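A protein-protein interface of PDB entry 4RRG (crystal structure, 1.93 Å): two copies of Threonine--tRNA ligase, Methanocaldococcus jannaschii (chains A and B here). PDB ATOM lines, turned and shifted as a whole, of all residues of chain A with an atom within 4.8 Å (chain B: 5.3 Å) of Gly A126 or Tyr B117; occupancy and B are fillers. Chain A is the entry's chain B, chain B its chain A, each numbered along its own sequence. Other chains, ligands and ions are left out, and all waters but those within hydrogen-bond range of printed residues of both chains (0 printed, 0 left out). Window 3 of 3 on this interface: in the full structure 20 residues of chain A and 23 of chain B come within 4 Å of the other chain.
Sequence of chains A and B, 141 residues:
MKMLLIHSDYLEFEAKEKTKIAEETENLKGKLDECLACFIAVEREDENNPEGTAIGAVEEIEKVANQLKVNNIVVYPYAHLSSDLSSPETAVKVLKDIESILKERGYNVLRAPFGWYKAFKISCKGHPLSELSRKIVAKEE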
ATOM      1  N   CYS A 124      28.843  23.534  15.737  1.00  0.00           N
ATOM      2  CA  CYS A 124      28.981  23.565  17.191  1.00  0.00           C
ATOM      3  C   CYS A 124      29.192  22.146  17.696  1.00  0.00           C
ATOM      4  O   CYS A 124      28.462  21.229  17.299  1.00  0.00           O
ATOM      5  CB  CYS A 124      27.709  24.124  17.835  1.00  0.00           C
ATOM      6  SG  CYS A 124      27.651  23.948  19.653  1.00  0.00           S
ATOM      7  N   LYS A 125      30.177  21.978  18.571  1.00  0.00           N
ATOM      8  CA  LYS A 125      30.553  20.658  19.105  1.00  0.00           C
ATOM      9  C   LYS A 125      29.480  20.009  19.996  1.00  0.00           C
ATOM     10  O   LYS A 125      29.396  18.780  20.096  1.00  0.00           O
ATOM     11  CB  LYS A 125      31.889  20.750  19.841  1.00  0.00           C
ATOM     12  CG  LYS A 125      33.048  21.037  18.906  1.00  0.00           C
ATOM     13  CD  LYS A 125      34.327  21.203  19.666  1.00  0.00           C
ATOM     14  CE  LYS A 125      35.500  21.438  18.723  1.00  0.00           C
ATOM     15  NZ  LYS A 125      35.758  20.222  17.898  1.00  0.00           N
ATOM     16  N   GLY A 126      28.646  20.814  20.638  1.00  0.00           N
ATOM     17  CA  GLY A 126      27.509  20.229  21.364  1.00  0.00           C
ATOM     18  C   GLY A 126      27.745  19.599  22.725  1.00  0.00           C
ATOM     19  O   GLY A 126      26.795  19.100  23.335  1.00  0.00           O
ATOM     20  N   HIS A 127      28.985  19.624  23.220  1.00  0.00           N
ATOM     21  CA  HIS A 127      29.267  19.232  24.616  1.00  0.00           C
ATOM     22  C   HIS A 127      28.711  20.279  25.607  1.00  0.00           C
ATOM     23  O   HIS A 127      28.307  21.360  25.188  1.00  0.00           O
ATOM     24  CB  HIS A 127      30.761  18.932  24.848  1.00  0.00           C
ATOM     25  CG  HIS A 127      31.669  20.106  24.629  1.00  0.00           C
ATOM     26  ND1 HIS A 127      31.802  21.126  25.543  1.00  0.00           N
ATOM     27  CD2 HIS A 127      32.513  20.401  23.613  1.00  0.00           C
ATOM     28  CE1 HIS A 127      32.670  22.015  25.089  1.00  0.00           C
ATOM     29  NE2 HIS A 127      33.118  21.596  23.919  1.00  0.00           N
ATOM     30  N   PRO A 128      28.644  19.950  26.913  1.00  0.00           N
ATOM     31  CA  PRO A 128      27.949  20.848  27.838  1.00  0.00           C
ATOM     32  C   PRO A 128      28.558  22.243  27.990  1.00  0.00           C
ATOM     33  O   PRO A 128      27.868  23.149  28.450  1.00  0.00           O
ATOM     34  CB  PRO A 128      27.990  20.085  29.166  1.00  0.00           C
ATOM     35  CG  PRO A 128      28.112  18.647  28.767  1.00  0.00           C
ATOM     36  CD  PRO A 128      29.005  18.674  27.562  1.00  0.00           C
ATOM     37  N   SER A 130      29.948  23.921  25.266  1.00  0.00           N
ATOM     38  CA  SER A 130      30.177  24.374  23.886  1.00  0.00           C
ATOM     39  C   SER A 130      29.399  25.625  23.492  1.00  0.00           C
ATOM     40  O   SER A 130      29.664  26.198  22.441  1.00  0.00           O
ATOM     41  CB  SER A 130      29.872  23.245  22.892  1.00  0.00           C
ATOM     42  OG  SER A 130      28.522  22.825  23.013  1.00  0.00           O
ATOM     43  N   GLU B  14      22.304  17.153  16.367  1.00  0.00           N
ATOM     44  CA  GLU B  14      22.479  15.841  16.964  1.00  0.00           C
ATOM     45  C   GLU B  14      22.509  15.995  18.472  1.00  0.00           C
ATOM     46  O   GLU B  14      23.458  16.543  19.020  1.00  0.00           O
ATOM     47  CB  GLU B  14      23.781  15.182  16.475  1.00  0.00           C
ATOM     48  CG  GLU B  14      24.088  13.836  17.156  1.00  0.00           C
ATOM     49  CD  GLU B  14      25.287  13.086  16.568  1.00  0.00           C
ATOM     50  OE1 GLU B  14      26.219  13.712  16.016  1.00  0.00           O
ATOM     51  OE2 GLU B  14      25.301  11.843  16.680  1.00  0.00           O
ATOM     52  N   ALA B  15      21.466  15.518  19.146  1.00  0.00           N
ATOM     53  CA  ALA B  15      21.465  15.517  20.607  1.00  0.00           C
ATOM     54  C   ALA B  15      22.621  14.645  21.074  1.00  0.00           C
ATOM     55  O   ALA B  15      22.888  13.593  20.486  1.00  0.00           O
ATOM     56  CB  ALA B  15      20.150  15.008  21.150  1.00  0.00           C
ATOM     57  N   LYS B  16      23.323  15.104  22.105  1.00  0.00           N
ATOM     58  CA  LYS B  16      24.504  14.413  22.604  1.00  0.00           C
ATOM     59  C   LYS B  16      24.386  14.050  24.075  1.00  0.00           C
ATOM     60  O   LYS B  16      24.850  12.986  24.497  1.00  0.00           O
ATOM     61  CB  LYS B  16      25.764  15.247  22.349  1.00  0.00           C
ATOM     62  CG  LYS B  16      26.239  15.171  20.911  1.00  0.00           C
ATOM     63  CD  LYS B  16      27.638  15.743  20.738  1.00  0.00           C
ATOM     64  CE  LYS B  16      28.149  15.521  19.314  1.00  0.00           C
ATOM     65  NZ  LYS B  16      28.448  14.088  19.003  1.00  0.00           N
ATOM     66  N   GLU B  17      23.755  14.922  24.856  1.00  0.00           N
ATOM     67  CA  GLU B  17      23.674  14.728  26.303  1.00  0.00           C
ATOM     68  C   GLU B  17      22.440  15.398  26.888  1.00  0.00           C
ATOM     69  O   GLU B  17      22.047  16.476  26.443  1.00  0.00           O
ATOM     70  CB  GLU B  17      24.935  15.284  26.969  1.00  0.00           C
ATOM     71  CG  GLU B  17      25.178  14.818  28.398  1.00  0.00           C
ATOM     72  CD  GLU B  17      26.593  15.107  28.869  1.00  0.00           C
ATOM     73  OE1 GLU B  17      27.529  15.029  28.047  1.00  0.00           O
ATOM     74  OE2 GLU B  17      26.771  15.409  30.063  1.00  0.00           O
ATOM     75  N   LYS B  18      21.835  14.749  27.884  1.00  0.00           N
ATOM     76  CA  LYS B  18      20.674  15.297  28.578  1.00  0.00           C
ATOM     77  C   LYS B  18      21.076  16.301  29.643  1.00  0.00           C
ATOM     78  O   LYS B  18      22.069  16.101  30.338  1.00  0.00           O
ATOM     79  CB  LYS B  18      19.862  14.178  29.249  1.00  0.00           C
ATOM     80  CG  LYS B  18      18.977  13.405  28.308  1.00  0.00           C
ATOM     81  CD  LYS B  18      17.937  12.549  29.032  1.00  0.00           C
ATOM     82  CE  LYS B  18      18.416  11.119  29.187  1.00  0.00           C
ATOM     83  NZ  LYS B  18      17.283  10.171  29.394  1.00  0.00           N
ATOM     84  N   THR B  19      20.296  17.376  29.762  1.00  0.00           N
ATOM     85  CA  THR B  19      20.311  18.222  30.956  1.00  0.00           C
ATOM     86  C   THR B  19      19.289  17.650  31.936  1.00  0.00           C
ATOM     87  O   THR B  19      18.632  16.657  31.635  1.00  0.00           O
ATOM     88  CB  THR B  19      19.909  19.688  30.659  1.00  0.00           C
ATOM     89  OG1 THR B  19      18.499  19.757  30.399  1.00  0.00           O
ATOM     90  CG2 THR B  19      20.692  20.256  29.482  1.00  0.00           C
ATOM     91  N   GLY B 115      16.083  20.926  26.016  1.00  0.00           N
ATOM     92  CA  GLY B 115      16.848  20.543  27.205  1.00  0.00           C
ATOM     93  C   GLY B 115      17.896  19.472  26.983  1.00  0.00           C
ATOM     94  O   GLY B 115      18.280  18.772  27.923  1.00  0.00           O
ATOM     95  N   TRP B 116      18.336  19.315  25.735  1.00  0.00           N
ATOM     96  CA  TRP B 116      19.465  18.447  25.414  1.00  0.00           C
ATOM     97  C   TRP B 116      20.606  19.308  24.896  1.00  0.00           C
ATOM     98  O   TRP B 116      20.364  20.279  24.179  1.00  0.00           O
ATOM     99  CB  TRP B 116      19.096  17.467  24.306  1.00  0.00           C
ATOM    100  CG  TRP B 116      18.097  16.394  24.659  1.00  0.00           C
ATOM    101  CD1 TRP B 116      16.756  16.549  24.852  1.00  0.00           C
ATOM    102  CD2 TRP B 116      18.368  14.997  24.811  1.00  0.00           C
ATOM    103  NE1 TRP B 116      16.171  15.329  25.118  1.00  0.00           N
ATOM    104  CE2 TRP B 116      17.140  14.362  25.104  1.00  0.00           C
ATOM    105  CE3 TRP B 116      19.535  14.220  24.737  1.00  0.00           C
ATOM    106  CZ2 TRP B 116      17.041  12.983  25.326  1.00  0.00           C
ATOM    107  CZ3 TRP B 116      19.435  12.847  24.956  1.00  0.00           C
ATOM    108  CH2 TRP B 116      18.196  12.243  25.244  1.00  0.00           C
ATOM    109  N   TYR B 117      21.843  18.956  25.252  1.00  0.00           N
ATOM    110  CA  TYR B 117      23.009  19.568  24.614  1.00  0.00           C
ATOM    111  C   TYR B 117      23.118  18.979  23.222  1.00  0.00           C
ATOM    112  O   TYR B 117      23.061  17.755  23.049  1.00  0.00           O
ATOM    113  CB  TYR B 117      24.296  19.285  25.388  1.00  0.00           C
ATOM    114  CG  TYR B 117      24.313  19.860  26.776  1.00  0.00           C
ATOM    115  CD1 TYR B 117      24.404  21.237  26.978  1.00  0.00           C
ATOM    116  CD2 TYR B 117      24.243  19.032  27.889  1.00  0.00           C
ATOM    117  CE1 TYR B 117      24.410  21.773  28.253  1.00  0.00           C
ATOM    118  CE2 TYR B 117      24.258  19.564  29.178  1.00  0.00           C
ATOM    119  CZ  TYR B 117      24.345  20.932  29.348  1.00  0.00           C
ATOM    120  OH  TYR B 117      24.356  21.475  30.613  1.00  0.00           O
ATOM    121  N   LYS B 118      23.269  19.845  22.230  1.00  0.00           N
ATOM    122  CA  LYS B 118      23.152  19.430  20.843  1.00  0.00           C
ATOM    123  C   LYS B 118      24.310  19.972  20.045  1.00  0.00           C
ATOM    124  O   LYS B 118      24.596  21.165  20.098  1.00  0.00           O
ATOM    125  CB  LYS B 118      21.863  19.984  20.221  1.00  0.00           C
ATOM    126  CG  LYS B 118      20.554  19.336  20.670  1.00  0.00           C
ATOM    127  CD  LYS B 118      19.347  20.081  20.075  1.00  0.00           C
ATOM    128  CE  LYS B 118      19.150  21.498  20.678  1.00  0.00           C
ATOM    129  NZ  LYS B 118      18.879  21.479  22.153  1.00  0.00           N
ATOM    130  N   ALA B 119      24.958  19.106  19.277  1.00  0.00           N
ATOM    131  CA  ALA B 119      25.838  19.591  18.217  1.00  0.00           C
ATOM    132  C   ALA B 119      24.931  20.063  17.097  1.00  0.00           C
ATOM    133  O   ALA B 119      23.834  19.517  16.912  1.00  0.00           O
ATOM    134  CB  ALA B 119      26.756  18.481  17.722  1.00  0.00           C
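The backbone NH (N) of Glu B14 is in hydrogen-bond range of the backbone carbonyl oxygen (O) of Ala B119 (2.9 Å).
The backbone carbonyl oxygen of Glu B17 lies within hydrogen-bond range of the backbone NH of Tyr B117, 2.8 Å away.
The side-chain amino group of Lys B118 sits at hydrogen-bond distance from the backbone carbonyl oxygen of Trp B116 (2.8 Å).
SG of Cys A124 sits close to N of Gly A126.
The side-chain sulfur of Cys A124 is in hydrogen-bond range of the side-chain hydroxyl of Ser A130, 3.6 Å away.
N of Gly A126 sits at hydrogen-bond distance from OG of Ser A130 (3.1 Å).
No position is printed for both chains.
Hydrophobic or aromatic side chains of chain A that line the printed part of chain B: Pro A128.
Printed residues of chain B that touch a printed residue of chain A: Lys B16, Glu B17, Tyr B117, Lys B118 and Ala B119.
Among the printed residues, 8 pairs touch across the chains.
Among the printed residues, no Asp or Glu carboxylate lies within 4 Å of a Lys or Arg side-chain nitrogen of the other chain.
Among the printed residues, pairs that only touch across the chains: Cys A124 with Ala B119, Lys A125 with Lys B16, Lys A125 with Ala B119, Gly A126 with Tyr B117, Gly A126 with Lys B118, Gly A126 with Ala B119, Pro A128 with Glu B17 and Pro A128 with Tyr B117.
Of the printed residues of chain B, Cys A124 touches Ala B119.
Gly A126 touches just these residues of chain B: Tyr B117 (3.2 Å), Lys B118 (3.3 Å) and Ala B119 (3.5 Å).
Of the printed residues of chain B, Pro A128 touches Glu B17 (3.7 Å) and Tyr B117 (3.7 Å).
Glu B14 touches none of the printed residues of chain A.
Ala B15 touches none of the printed residues of chain A.
Printed residues of chain A within 4 Å of Glu B17: Pro A128 (3.7 Å).
The nearest residue of chain A that does not touch Tyr B117 is His A127 (4.3 Å).
The nearest printed residue of chain A that does not touch Glu B17 is Gly A126 (5.4 Å).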
